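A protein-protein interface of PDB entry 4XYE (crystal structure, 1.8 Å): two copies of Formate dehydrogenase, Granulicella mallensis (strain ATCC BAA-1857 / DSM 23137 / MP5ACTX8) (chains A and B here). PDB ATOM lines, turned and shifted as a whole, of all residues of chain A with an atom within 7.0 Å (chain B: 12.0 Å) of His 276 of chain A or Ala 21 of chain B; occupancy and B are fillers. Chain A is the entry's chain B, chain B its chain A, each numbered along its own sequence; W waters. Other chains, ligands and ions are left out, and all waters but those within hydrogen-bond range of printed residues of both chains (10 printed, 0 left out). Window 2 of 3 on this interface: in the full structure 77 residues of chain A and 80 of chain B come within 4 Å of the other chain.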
ATOM      1  N   SER A 185      -7.585 -10.816 -23.436  1.00  0.00           N
ATOM      2  CA  SER A 185      -8.665  -9.858 -23.193  1.00  0.00           C
ATOM      3  C   SER A 185      -9.715 -10.384 -22.211  1.00  0.00           C
ATOM      4  O   SER A 185     -10.423  -9.600 -21.584  1.00  0.00           O
ATOM      5  CB  SER A 185      -9.318  -9.428 -24.509  1.00  0.00           C
ATOM      6  OG  SER A 185      -8.485  -8.485 -25.156  1.00  0.00           O
ATOM      7  N   ARG A 186      -9.802 -11.707 -22.075  1.00  0.00           N
ATOM      8  CA  ARG A 186     -10.682 -12.326 -21.085  1.00  0.00           C
ATOM      9  C   ARG A 186      -9.916 -13.293 -20.181  1.00  0.00           C
ATOM     10  O   ARG A 186     -10.498 -14.242 -19.668  1.00  0.00           O
ATOM     11  CB  ARG A 186     -11.818 -13.122 -21.765  1.00  0.00           C
ATOM     12  CG  ARG A 186     -12.608 -12.417 -22.840  1.00  0.00           C
ATOM     13  CD  ARG A 186     -13.518 -13.447 -23.534  1.00  0.00           C
ATOM     14  NE  ARG A 186     -14.344 -14.174 -22.560  1.00  0.00           N
ATOM     15  CZ  ARG A 186     -15.401 -13.635 -21.959  1.00  0.00           C
ATOM     16  NH1 ARG A 186     -15.752 -12.390 -22.246  1.00  0.00           N
ATOM     17  NH2 ARG A 186     -16.114 -14.329 -21.090  1.00  0.00           N
ATOM     18  N   TYR A 188      -7.852 -14.202 -16.766  1.00  0.00           N
ATOM     19  CA  TYR A 188      -7.585 -13.799 -15.385  1.00  0.00           C
ATOM     20  C   TYR A 188      -6.875 -14.908 -14.630  1.00  0.00           C
ATOM     21  O   TYR A 188      -6.928 -16.067 -15.039  1.00  0.00           O
ATOM     22  CB  TYR A 188      -8.887 -13.460 -14.649  1.00  0.00           C
ATOM     23  CG  TYR A 188      -9.637 -12.301 -15.265  1.00  0.00           C
ATOM     24  CD1 TYR A 188      -9.316 -10.993 -14.934  1.00  0.00           C
ATOM     25  CD2 TYR A 188     -10.657 -12.516 -16.181  1.00  0.00           C
ATOM     26  CE1 TYR A 188      -9.991  -9.922 -15.498  1.00  0.00           C
ATOM     27  CE2 TYR A 188     -11.350 -11.445 -16.756  1.00  0.00           C
ATOM     28  CZ  TYR A 188     -11.006 -10.152 -16.404  1.00  0.00           C
ATOM     29  OH  TYR A 188     -11.666  -9.085 -16.967  1.00  0.00           O
ATOM     30  N   LEU A 271     -28.431 -17.385 -10.308  1.00  0.00           N
ATOM     31  CA  LEU A 271     -27.445 -16.846 -11.242  1.00  0.00           C
ATOM     32  C   LEU A 271     -27.365 -15.322 -11.161  1.00  0.00           C
ATOM     33  O   LEU A 271     -26.272 -14.750 -11.163  1.00  0.00           O
ATOM     34  CB  LEU A 271     -27.784 -17.271 -12.672  1.00  0.00           C
ATOM     35  CG  LEU A 271     -27.751 -18.773 -12.947  1.00  0.00           C
ATOM     36  CD1 LEU A 271     -28.329 -19.082 -14.330  1.00  0.00           C
ATOM     37  CD2 LEU A 271     -26.333 -19.300 -12.826  1.00  0.00           C
ATOM     38  N   ASN A 272     -28.518 -14.662 -11.074  1.00  0.00           N
ATOM     39  CA  ASN A 272     -28.529 -13.200 -11.003  1.00  0.00           C
ATOM     40  C   ASN A 272     -27.994 -12.620  -9.687  1.00  0.00           C
ATOM     41  O   ASN A 272     -27.705 -11.424  -9.607  1.00  0.00           O
ATOM     42  CB  ASN A 272     -29.907 -12.631 -11.352  1.00  0.00           C
ATOM     43  CG  ASN A 272     -30.285 -12.890 -12.802  1.00  0.00           C
ATOM     44  OD1 ASN A 272     -29.411 -13.087 -13.655  1.00  0.00           O
ATOM     45  ND2 ASN A 272     -31.582 -12.924 -13.084  1.00  0.00           N
ATOM     46  N   LYS A 273     -27.839 -13.463  -8.670  1.00  0.00           N
ATOM     47  CA  LYS A 273     -27.216 -13.022  -7.425  1.00  0.00           C
ATOM     48  C   LYS A 273     -25.704 -12.933  -7.588  1.00  0.00           C
ATOM     49  O   LYS A 273     -25.029 -12.263  -6.810  1.00  0.00           O
ATOM     50  CB  LYS A 273     -27.519 -13.981  -6.273  1.00  0.00           C
ATOM     51  CG  LYS A 273     -28.973 -14.072  -5.873  1.00  0.00           C
ATOM     52  CD  LYS A 273     -29.335 -13.054  -4.824  1.00  0.00           C
ATOM     53  CE  LYS A 273     -30.680 -13.402  -4.195  1.00  0.00           C
ATOM     54  NZ  LYS A 273     -31.098 -12.379  -3.198  1.00  0.00           N
ATOM     55  N   MET A 274     -25.166 -13.639  -8.577  1.00  0.00           N
ATOM     56  CA  MET A 274     -23.727 -13.602  -8.796  1.00  0.00           C
ATOM     57  C   MET A 274     -23.360 -12.270  -9.409  1.00  0.00           C
ATOM     58  O   MET A 274     -24.178 -11.623 -10.078  1.00  0.00           O
ATOM     59  CB  MET A 274     -23.264 -14.750  -9.696  1.00  0.00           C
ATOM     60  CG  MET A 274     -23.581 -16.121  -9.149  1.00  0.00           C
ATOM     61  SD  MET A 274     -22.768 -17.444 -10.070  1.00  0.00           S
ATOM     62  CE  MET A 274     -21.152 -17.451  -9.293  1.00  0.00           C
ATOM     63  N   ARG A 275     -22.137 -11.841  -9.164  1.00  0.00           N
ATOM     64  CA  ARG A 275     -21.640 -10.638  -9.808  1.00  0.00           C
ATOM     65  C   ARG A 275     -21.471 -10.889 -11.303  1.00  0.00           C
ATOM     66  O   ARG A 275     -21.060 -11.977 -11.720  1.00  0.00           O
ATOM     67  CB  ARG A 275     -20.309 -10.216  -9.187  1.00  0.00           C
ATOM     68  CG  ARG A 275     -19.741  -8.938  -9.766  1.00  0.00           C
ATOM     69  CD  ARG A 275     -18.639  -8.397  -8.871  1.00  0.00           C
ATOM     70  NE  ARG A 275     -19.069  -8.385  -7.478  1.00  0.00           N
ATOM     71  CZ  ARG A 275     -19.581  -7.324  -6.861  1.00  0.00           C
ATOM     72  NH1 ARG A 275     -19.720  -6.177  -7.515  1.00  0.00           N
ATOM     73  NH2 ARG A 275     -19.951  -7.409  -5.588  1.00  0.00           N
ATOM     74  N   HIS A 276     -21.792  -9.883 -12.107  1.00  0.00           N
ATOM     75  CA  HIS A 276     -21.583  -9.959 -13.546  1.00  0.00           C
ATOM     76  C   HIS A 276     -20.146 -10.406 -13.875  1.00  0.00           C
ATOM     77  O   HIS A 276     -19.177  -9.808 -13.402  1.00  0.00           O
ATOM     78  CB  HIS A 276     -21.864  -8.591 -14.175  1.00  0.00           C
ATOM     79  CG  HIS A 276     -21.654  -8.552 -15.655  1.00  0.00           C
ATOM     80  ND1 HIS A 276     -22.681  -8.734 -16.561  1.00  0.00           N
ATOM     81  CD2 HIS A 276     -20.537  -8.349 -16.395  1.00  0.00           C
ATOM     82  CE1 HIS A 276     -22.207  -8.641 -17.788  1.00  0.00           C
ATOM     83  NE2 HIS A 276     -20.907  -8.410 -17.717  1.00  0.00           N
ATOM     84  N   GLY A 277     -20.017 -11.453 -14.686  1.00  0.00           N
ATOM     85  CA  GLY A 277     -18.706 -11.948 -15.075  1.00  0.00           C
ATOM     86  C   GLY A 277     -18.215 -13.098 -14.204  1.00  0.00           C
ATOM     87  O   GLY A 277     -17.026 -13.413 -14.190  1.00  0.00           O
ATOM     88  N   SER A 278     -19.127 -13.726 -13.471  1.00  0.00           N
ATOM     89  CA  SER A 278     -18.757 -14.855 -12.618  1.00  0.00           C
ATOM     90  C   SER A 278     -18.684 -16.155 -13.431  1.00  0.00           C
ATOM     91  O   SER A 278     -19.056 -16.187 -14.614  1.00  0.00           O
ATOM     92  CB  SER A 278     -19.744 -14.983 -11.445  1.00  0.00           C
ATOM     93  OG  SER A 278     -19.636 -13.873 -10.554  1.00  0.00           O
ATOM     94  N   TYR A 279     -18.185 -17.220 -12.799  1.00  0.00           N
ATOM     95  CA  TYR A 279     -17.968 -18.493 -13.476  1.00  0.00           C
ATOM     96  C   TYR A 279     -18.687 -19.617 -12.753  1.00  0.00           C
ATOM     97  O   TYR A 279     -18.742 -19.632 -11.528  1.00  0.00           O
ATOM     98  CB  TYR A 279     -16.472 -18.828 -13.514  1.00  0.00           C
ATOM     99  CG  TYR A 279     -15.645 -17.806 -14.270  1.00  0.00           C
ATOM    100  CD1 TYR A 279     -15.134 -16.690 -13.619  1.00  0.00           C
ATOM    101  CD2 TYR A 279     -15.393 -17.948 -15.635  1.00  0.00           C
ATOM    102  CE1 TYR A 279     -14.383 -15.744 -14.296  1.00  0.00           C
ATOM    103  CE2 TYR A 279     -14.637 -16.999 -16.330  1.00  0.00           C
ATOM    104  CZ  TYR A 279     -14.137 -15.900 -15.649  1.00  0.00           C
ATOM    105  OH  TYR A 279     -13.395 -14.954 -16.323  1.00  0.00           O
ATOM    106  N   ALA A 297     -27.546 -16.635 -19.413  1.00  0.00           N
ATOM    107  CA  ALA A 297     -26.545 -16.000 -18.568  1.00  0.00           C
ATOM    108  C   ALA A 297     -25.224 -15.790 -19.321  1.00  0.00           C
ATOM    109  O   ALA A 297     -24.558 -14.775 -19.145  1.00  0.00           O
ATOM    110  CB  ALA A 297     -26.316 -16.816 -17.299  1.00  0.00           C
ATOM    111  N   SER A 300     -25.680 -13.000 -22.063  1.00  0.00           N
ATOM    112  CA  SER A 300     -25.728 -11.643 -21.493  1.00  0.00           C
ATOM    113  C   SER A 300     -24.448 -11.227 -20.777  1.00  0.00           C
ATOM    114  O   SER A 300     -24.262 -10.053 -20.461  1.00  0.00           O
ATOM    115  CB  SER A 300     -26.882 -11.520 -20.503  1.00  0.00           C
ATOM    116  OG  SER A 300     -26.570 -12.187 -19.288  1.00  0.00           O
ATOM    117  N   GLY A 301     -23.575 -12.191 -20.500  1.00  0.00           N
ATOM    118  CA  GLY A 301     -22.339 -11.913 -19.792  1.00  0.00           C
ATOM    119  C   GLY A 301     -22.499 -11.973 -18.282  1.00  0.00           C
ATOM    120  O   GLY A 301     -21.554 -11.703 -17.544  1.00  0.00           O
ATOM    121  N   GLN A 302     -23.698 -12.319 -17.820  1.00  0.00           N
ATOM    122  CA  GLN A 302     -23.921 -12.508 -16.391  1.00  0.00           C
ATOM    123  C   GLN A 302     -22.956 -13.566 -15.854  1.00  0.00           C
ATOM    124  O   GLN A 302     -22.314 -13.376 -14.820  1.00  0.00           O
ATOM    125  CB  GLN A 302     -25.371 -12.903 -16.109  1.00  0.00           C
ATOM    126  CG  GLN A 302     -25.639 -13.206 -14.641  1.00  0.00           C
ATOM    127  CD  GLN A 302     -25.465 -11.978 -13.735  1.00  0.00           C
ATOM    128  OE1 GLN A 302     -25.460 -10.836 -14.201  1.00  0.00           O
ATOM    129  NE2 GLN A 302     -25.328 -12.218 -12.437  1.00  0.00           N
ATOM    130  N   LEU A 303     -22.848 -14.676 -16.575  1.00  0.00           N
ATOM    131  CA  LEU A 303     -21.709 -15.573 -16.415  1.00  0.00           C
ATOM    132  C   LEU A 303     -20.666 -15.248 -17.480  1.00  0.00           C
ATOM    133  O   LEU A 303     -21.001 -15.086 -18.654  1.00  0.00           O
ATOM    134  CB  LEU A 303     -22.137 -17.041 -16.564  1.00  0.00           C
ATOM    135  CG  LEU A 303     -22.990 -17.642 -15.454  1.00  0.00           C
ATOM    136  CD1 LEU A 303     -23.372 -19.084 -15.821  1.00  0.00           C
ATOM    137  CD2 LEU A 303     -22.223 -17.620 -14.155  1.00  0.00           C
ATOM    138  N   ALA A 304     -19.402 -15.154 -17.069  1.00  0.00           N
ATOM    139  CA  ALA A 304     -18.291 -15.048 -18.004  1.00  0.00           C
ATOM    140  C   ALA A 304     -17.937 -16.423 -18.587  1.00  0.00           C
ATOM    141  O   ALA A 304     -17.325 -16.511 -19.645  1.00  0.00           O
ATOM    142  CB  ALA A 304     -17.069 -14.437 -17.318  1.00  0.00           C
ATOM    143  N   HIS A 327     -18.643 -19.022 -24.628  1.00  0.00           N
ATOM    144  CA  HIS A 327     -17.752 -19.079 -23.482  1.00  0.00           C
ATOM    145  C   HIS A 327     -17.979 -20.329 -22.647  1.00  0.00           C
ATOM    146  O   HIS A 327     -18.076 -20.260 -21.419  1.00  0.00           O
ATOM    147  CB  HIS A 327     -17.955 -17.831 -22.624  1.00  0.00           C
ATOM    148  CG  HIS A 327     -17.711 -16.552 -23.361  1.00  0.00           C
ATOM    149  ND1 HIS A 327     -18.459 -15.413 -23.149  1.00  0.00           N
ATOM    150  CD2 HIS A 327     -16.798 -16.233 -24.310  1.00  0.00           C
ATOM    151  CE1 HIS A 327     -18.020 -14.450 -23.939  1.00  0.00           C
ATOM    152  NE2 HIS A 327     -17.016 -14.920 -24.655  1.00  0.00           N
ATOM    153  N   PRO B  12      -6.388  -5.709 -29.524  1.00  0.00           N
ATOM    154  CA  PRO B  12      -7.325  -6.786 -29.881  1.00  0.00           C
ATOM    155  C   PRO B  12      -7.944  -6.568 -31.254  1.00  0.00           C
ATOM    156  O   PRO B  12      -8.124  -5.424 -31.692  1.00  0.00           O
ATOM    157  CB  PRO B  12      -8.433  -6.664 -28.829  1.00  0.00           C
ATOM    158  CG  PRO B  12      -7.813  -5.931 -27.674  1.00  0.00           C
ATOM    159  CD  PRO B  12      -6.767  -5.028 -28.270  1.00  0.00           C
ATOM    160  N   SER B  14     -10.972  -6.947 -32.098  1.00  0.00           N
ATOM    161  CA  SER B  14     -12.257  -6.271 -31.947  1.00  0.00           C
ATOM    162  C   SER B  14     -12.115  -4.772 -31.692  1.00  0.00           C
ATOM    163  O   SER B  14     -13.090  -4.029 -31.784  1.00  0.00           O
ATOM    164  CB  SER B  14     -13.067  -6.906 -30.812  1.00  0.00           C
ATOM    165  OG  SER B  14     -12.488  -6.621 -29.547  1.00  0.00           O
ATOM    166  N   GLY B  15     -10.904  -4.332 -31.364  1.00  0.00           N
ATOM    167  CA  GLY B  15     -10.661  -2.941 -31.034  1.00  0.00           C
ATOM    168  C   GLY B  15     -10.211  -2.718 -29.597  1.00  0.00           C
ATOM    169  O   GLY B  15     -10.243  -3.629 -28.767  1.00  0.00           O
ATOM    170  N   PRO B  17     -10.649  -0.021 -26.211  1.00  0.00           N
ATOM    171  CA  PRO B  17     -10.436  -1.128 -25.264  1.00  0.00           C
ATOM    172  C   PRO B  17     -11.325  -2.310 -25.575  1.00  0.00           C
ATOM    173  O   PRO B  17     -12.319  -2.146 -26.276  1.00  0.00           O
ATOM    174  CB  PRO B  17     -10.857  -0.522 -23.920  1.00  0.00           C
ATOM    175  CG  PRO B  17     -11.821   0.541 -24.279  1.00  0.00           C
ATOM    176  CD  PRO B  17     -11.312   1.125 -25.565  1.00  0.00           C
ATOM    177  N   PRO B  18     -10.973  -3.493 -25.059  1.00  0.00           N
ATOM    178  CA  PRO B  18     -11.867  -4.638 -25.211  1.00  0.00           C
ATOM    179  C   PRO B  18     -13.062  -4.493 -24.283  1.00  0.00           C
ATOM    180  O   PRO B  18     -13.052  -3.673 -23.360  1.00  0.00           O
ATOM    181  CB  PRO B  18     -11.005  -5.821 -24.750  1.00  0.00           C
ATOM    182  CG  PRO B  18     -10.033  -5.233 -23.797  1.00  0.00           C
ATOM    183  CD  PRO B  18      -9.757  -3.828 -24.292  1.00  0.00           C
ATOM    184  N   LEU B  19     -14.080  -5.301 -24.533  1.00  0.00           N
ATOM    185  CA  LEU B  19     -15.219  -5.399 -23.638  1.00  0.00           C
ATOM    186  C   LEU B  19     -14.850  -6.342 -22.492  1.00  0.00           C
ATOM    187  O   LEU B  19     -14.794  -7.554 -22.669  1.00  0.00           O
ATOM    188  CB  LEU B  19     -16.426  -5.950 -24.399  1.00  0.00           C
ATOM    189  CG  LEU B  19     -17.736  -5.957 -23.617  1.00  0.00           C
ATOM    190  CD1 LEU B  19     -18.105  -4.538 -23.225  1.00  0.00           C
ATOM    191  CD2 LEU B  19     -18.847  -6.616 -24.425  1.00  0.00           C
ATOM    192  N   TYR B  20     -14.584  -5.779 -21.321  1.00  0.00           N
ATOM    193  CA  TYR B  20     -14.135  -6.578 -20.183  1.00  0.00           C
ATOM    194  C   TYR B  20     -15.273  -7.418 -19.611  1.00  0.00           C
ATOM    195  O   TYR B  20     -16.408  -6.934 -19.479  1.00  0.00           O
ATOM    196  CB  TYR B  20     -13.571  -5.667 -19.100  1.00  0.00           C
ATOM    197  CG  TYR B  20     -12.374  -4.878 -19.571  1.00  0.00           C
ATOM    198  CD1 TYR B  20     -11.160  -5.511 -19.816  1.00  0.00           C
ATOM    199  CD2 TYR B  20     -12.459  -3.509 -19.787  1.00  0.00           C
ATOM    200  CE1 TYR B  20     -10.049  -4.800 -20.244  1.00  0.00           C
ATOM    201  CE2 TYR B  20     -11.359  -2.790 -20.228  1.00  0.00           C
ATOM    202  CZ  TYR B  20     -10.159  -3.444 -20.457  1.00  0.00           C
ATOM    203  OH  TYR B  20      -9.060  -2.748 -20.889  1.00  0.00           O
ATOM    204  N   ALA B  21     -14.954  -8.659 -19.251  1.00  0.00           N
ATOM    205  CA  ALA B  21     -15.933  -9.579 -18.691  1.00  0.00           C
ATOM    206  C   ALA B  21     -16.336  -9.221 -17.267  1.00  0.00           C
ATOM    207  O   ALA B  21     -17.445  -9.559 -16.831  1.00  0.00           O
ATOM    208  CB  ALA B  21     -15.402 -11.018 -18.752  1.00  0.00           C
ATOM    209  N   ARG B  22     -15.436  -8.551 -16.542  1.00  0.00           N
ATOM    210  CA  ARG B  22     -15.680  -8.165 -15.150  1.00  0.00           C
ATOM    211  C   ARG B  22     -15.065  -6.799 -14.885  1.00  0.00           C
ATOM    212  O   ARG B  22     -14.184  -6.365 -15.621  1.00  0.00           O
ATOM    213  CB  ARG B  22     -15.099  -9.194 -14.166  1.00  0.00           C
ATOM    214  CG  ARG B  22     -13.559  -9.286 -14.187  1.00  0.00           C
ATOM    215  CD  ARG B  22     -13.040 -10.350 -13.188  1.00  0.00           C
ATOM    216  NE  ARG B  22     -13.953 -11.484 -13.082  1.00  0.00           N
ATOM    217  CZ  ARG B  22     -14.403 -11.969 -11.933  1.00  0.00           C
ATOM    218  NH1 ARG B  22     -14.028 -11.411 -10.776  1.00  0.00           N
ATOM    219  NH2 ARG B  22     -15.230 -12.998 -11.933  1.00  0.00           N
ATOM    220  N   ASN B  23     -15.511  -6.132 -13.823  1.00  0.00           N
ATOM    221  CA  ASN B  23     -15.089  -4.752 -13.596  1.00  0.00           C
ATOM    222  C   ASN B  23     -13.989  -4.575 -12.550  1.00  0.00           C
ATOM    223  O   ASN B  23     -13.472  -3.467 -12.351  1.00  0.00           O
ATOM    224  CB  ASN B  23     -16.299  -3.867 -13.280  1.00  0.00           C
ATOM    225  CG  ASN B  23     -16.904  -4.155 -11.916  1.00  0.00           C
ATOM    226  OD1 ASN B  23     -16.714  -5.230 -11.340  1.00  0.00           O
ATOM    227  ND2 ASN B  23     -17.645  -3.187 -11.393  1.00  0.00           N
ATOM    228  N   ALA B  24     -13.592  -5.666 -11.907  1.00  0.00           N
ATOM    229  CA  ALA B  24     -12.521  -5.600 -10.914  1.00  0.00           C
ATOM    230  C   ALA B  24     -11.787  -6.930 -10.827  1.00  0.00           C
ATOM    231  O   ALA B  24     -12.323  -7.961 -11.225  1.00  0.00           O
ATOM    232  CB  ALA B  24     -13.089  -5.230  -9.550  1.00  0.00           C
ATOM    233  N   ILE B  25     -10.562  -6.891 -10.305  1.00  0.00           N
ATOM    234  CA  ILE B  25      -9.788  -8.104 -10.032  1.00  0.00           C
ATOM    235  C   ILE B  25      -9.324  -8.103  -8.573  1.00  0.00           C
ATOM    236  O   ILE B  25      -9.346  -7.046  -7.911  1.00  0.00           O
ATOM    237  CB  ILE B  25      -8.572  -8.225 -10.988  1.00  0.00           C
ATOM    238  CG1 ILE B  25      -7.635  -7.032 -10.825  1.00  0.00           C
ATOM    239  CG2 ILE B  25      -9.049  -8.360 -12.429  1.00  0.00           C
ATOM    240  CD1 ILE B  25      -6.334  -7.173 -11.591  1.00  0.00           C
ATOM    241  N   PRO B  26      -8.921  -9.279  -8.051  1.00  0.00           N
ATOM    242  CA  PRO B  26      -8.501  -9.366  -6.648  1.00  0.00           C
ATOM    243  C   PRO B  26      -7.312  -8.467  -6.327  1.00  0.00           C
ATOM    244  O   PRO B  26      -6.523  -8.125  -7.202  1.00  0.00           O
ATOM    245  CB  PRO B  26      -8.106 -10.839  -6.498  1.00  0.00           C
ATOM    246  CG  PRO B  26      -8.973 -11.541  -7.465  1.00  0.00           C
ATOM    247  CD  PRO B  26      -9.019 -10.619  -8.660  1.00  0.00           C
ATOM    248  N   VAL B  46      -6.534   1.327 -14.100  1.00  0.00           N
ATOM    249  CA  VAL B  46      -7.299   0.549 -13.130  1.00  0.00           C
ATOM    250  C   VAL B  46      -6.880  -0.916 -13.276  1.00  0.00           C
ATOM    251  O   VAL B  46      -6.933  -1.440 -14.379  1.00  0.00           O
ATOM    252  CB  VAL B  46      -8.814   0.657 -13.408  1.00  0.00           C
ATOM    253  CG1 VAL B  46      -9.596  -0.235 -12.442  1.00  0.00           C
ATOM    254  CG2 VAL B  46      -9.278   2.130 -13.345  1.00  0.00           C
ATOM    255  N   PRO B  47      -6.441  -1.572 -12.177  1.00  0.00           N
ATOM    256  CA  PRO B  47      -6.050  -2.980 -12.315  1.00  0.00           C
ATOM    257  C   PRO B  47      -7.177  -3.773 -12.959  1.00  0.00           C
ATOM    258  O   PRO B  47      -8.333  -3.625 -12.562  1.00  0.00           O
ATOM    259  CB  PRO B  47      -5.843  -3.428 -10.867  1.00  0.00           C
ATOM    260  CG  PRO B  47      -5.344  -2.158 -10.186  1.00  0.00           C
ATOM    261  CD  PRO B  47      -6.215  -1.075 -10.805  1.00  0.00           C
ATOM    262  N   GLY B  48      -6.842  -4.569 -13.967  1.00  0.00           N
ATOM    263  CA  GLY B  48      -7.854  -5.282 -14.722  1.00  0.00           C
ATOM    264  C   GLY B  48      -7.912  -4.807 -16.158  1.00  0.00           C
ATOM    265  O   GLY B  48      -8.406  -5.512 -17.038  1.00  0.00           O
ATOM    266  N   GLU B  49      -7.407  -3.608 -16.413  1.00  0.00           N
ATOM    267  CA  GLU B  49      -7.377  -3.099 -17.783  1.00  0.00           C
ATOM    268  C   GLU B  49      -6.307  -3.778 -18.648  1.00  0.00           C
ATOM    269  O   GLU B  49      -5.312  -4.303 -18.144  1.00  0.00           O
ATOM    270  CB  GLU B  49      -7.186  -1.582 -17.780  1.00  0.00           C
ATOM    271  CG  GLU B  49      -8.426  -0.851 -17.242  1.00  0.00           C
ATOM    272  CD  GLU B  49      -8.307   0.673 -17.235  1.00  0.00           C
ATOM    273  OE1 GLU B  49      -7.228   1.197 -16.917  1.00  0.00           O
ATOM    274  OE2 GLU B  49      -9.316   1.353 -17.527  1.00  0.00           O
ATOM    275  N   LEU B  50      -6.520  -3.775 -19.956  1.00  0.00           N
ATOM    276  CA  LEU B  50      -5.535  -4.334 -20.875  1.00  0.00           C
ATOM    277  C   LEU B  50      -4.434  -3.307 -21.102  1.00  0.00           C
ATOM    278  O   LEU B  50      -4.680  -2.217 -21.632  1.00  0.00           O
ATOM    279  CB  LEU B  50      -6.189  -4.710 -22.203  1.00  0.00           C
ATOM    280  CG  LEU B  50      -5.279  -5.284 -23.281  1.00  0.00           C
ATOM    281  CD1 LEU B  50      -4.611  -6.577 -22.793  1.00  0.00           C
ATOM    282  CD2 LEU B  50      -6.085  -5.548 -24.562  1.00  0.00           C
ATOM    283  N   SER B 338      -1.955 -12.470 -18.366  1.00  0.00           N
ATOM    284  CA  SER B 338      -3.332 -12.398 -17.895  1.00  0.00           C
ATOM    285  C   SER B 338      -3.530 -10.969 -17.417  1.00  0.00           C
ATOM    286  O   SER B 338      -2.573 -10.309 -17.040  1.00  0.00           O
ATOM    287  CB  SER B 338      -3.569 -13.361 -16.738  1.00  0.00           C
ATOM    288  OG  SER B 338      -2.880 -12.924 -15.578  1.00  0.00           O
ATOM    289  N   LEU B 339      -4.757 -10.477 -17.440  1.00  0.00           N
ATOM    290  CA  LEU B 339      -4.993  -9.096 -17.005  1.00  0.00           C
ATOM    291  C   LEU B 339      -4.517  -8.890 -15.559  1.00  0.00           C
ATOM    292  O   LEU B 339      -4.007  -7.824 -15.205  1.00  0.00           O
ATOM    293  CB  LEU B 339      -6.481  -8.760 -17.160  1.00  0.00           C
ATOM    294  CG  LEU B 339      -6.967  -8.768 -18.614  1.00  0.00           C
ATOM    295  CD1 LEU B 339      -8.508  -8.724 -18.682  1.00  0.00           C
ATOM    296  CD2 LEU B 339      -6.341  -7.623 -19.433  1.00  0.00           C
ATOM    297  N   SER B 340      -4.646  -9.931 -14.740  1.00  0.00           N
ATOM    298  CA  SER B 340      -4.224  -9.869 -13.343  1.00  0.00           C
ATOM    299  C   SER B 340      -2.713  -9.691 -13.285  1.00  0.00           C
ATOM    300  O   SER B 340      -2.187  -8.901 -12.494  1.00  0.00           O
ATOM    301  CB  SER B 340      -4.628 -11.151 -12.594  1.00  0.00           C
ATOM    302  OG  SER B 340      -5.955 -11.550 -12.937  1.00  0.00           O
HETATM  303  O   HOH W   1     -12.363  -9.437 -19.612  1.00  0.00           O
HETATM  304  O   HOH W   2     -10.750  -6.788 -16.225  1.00  0.00           O
HETATM  305  O   HOH W   3     -17.264 -12.511 -10.230  1.00  0.00           O
HETATM  306  O   HOH W   4     -19.026  -7.989 -20.119  1.00  0.00           O
HETATM  307  O   HOH W   5     -16.420  -9.751 -22.458  1.00  0.00           O
HETATM  308  O   HOH W   6     -18.299  -7.190 -13.003  1.00  0.00           O
HETATM  309  O   HOH W   7     -11.084  -8.428 -27.316  1.00  0.00           O
HETATM  310  O   HOH W   8     -19.051 -11.338 -18.396  1.00  0.00           O
HETATM  311  O   HOH W   9     -14.655 -12.551 -15.352  1.00  0.00           O
HETATM  312  O   HOH W  10     -17.188 -10.180 -11.483  1.00  0.00           O
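Water W2 bridges OH of Tyr 188 of chain A (2.6 Å) and O of Gly 48 of chain B (2.8 Å). Water W3 lies within hydrogen-bond range of the guanidinium group (NH2) of Arg 22 of chain B and the side-chain hydroxyl (OG) of Ser 278 of chain A. Water W4 lies within hydrogen-bond range of the backbone carbonyl oxygen (O) of Tyr 20 of chain B (2.9 Å) and a ring nitrogen (NE2) of His 276 of chain A (3.1 Å).
Of the 19 printed residues of chain A, 6 touch a printed residue of chain B. Printed residues of chain B that touch a printed residue of chain A: Pro 12, Pro 18, Ala 21, Arg 22, Ile 25, Leu 50, Leu 339 and Ser 340. Among the printed residues, 13 pairs touch across the chains.
No position is printed for both chains. Of the 13 pairs that touch across the chains among the printed residues, none has its exchanged pair printed and touching as well.
The guanidinium group (NH2) of Arg 22 of chain B is in hydrogen-bond range of the backbone carbonyl oxygen (O) of Gly 277 of chain A (2.9 Å).
Of chain B, only Ala 21 comes within 4 Å of Arg 186 of chain A. No residue of chain B comes within 4 Å of Arg 275 of chain A. Of chain B, only Ala 21 (3.3 Å) comes within 4 Å of His 276 of chain A. Ser 278 of chain A touches none of the printed residues of chain B. Ser 300 of chain A touches none of the printed residues of chain B. No residue of chain B comes within 4 Å of Gly 301 of chain A. No residue of chain B comes within 4 Å of Gln 302 of chain A. No residue of chain B comes within 4 Å of Ala 304 of chain A. Of the printed residues of chain A, Ile 25 of chain B touches Tyr 188 (3.6 Å). Of the printed residues of chain A, Leu 50 of chain B touches Ser 185. Ser 338 of chain B touches none of the printed residues of chain A. The nearest residue of chain B that does not touch His 276 of chain A is Arg 22 of chain B (4.2 Å).
The side-chain hydroxyl (OH) of Tyr 20 of chain B is in hydrogen-bond range of the backbone NH (N) of Leu 50 of chain B (2.9 Å). The backbone NH (N) of Gly 277 of chain A is in hydrogen-bond range of the backbone carbonyl oxygen (O) of Gly 301 of chain A (3.3 Å). N of Gly 277 of chain A is in hydrogen-bond range of O of Gln 302 of chain A (3.0 Å).
Among the printed residues, merely in contact across the chains: Gly 277 of chain A with Ala 21 of chain B, His 276 of chain A with Ala 21 of chain B, Tyr 188 of chain A with Arg 22 of chain B, Tyr 188 of chain A with Ile 25 of chain B, Ser 185 of chain A with Leu 339 of chain B, Tyr 188 of chain A with Leu 339 of chain B, Ser 185 of chain A with Pro 12 of chain B, Ser 185 of chain A with Pro 18 of chain B, Tyr 188 of chain A with Ser 340 of chain B, Tyr 279 of chain A with Arg 22 of chain B, Arg 186 of chain A with Ala 21 of chain B and Ser 185 of chain A with Leu 50 of chain B.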
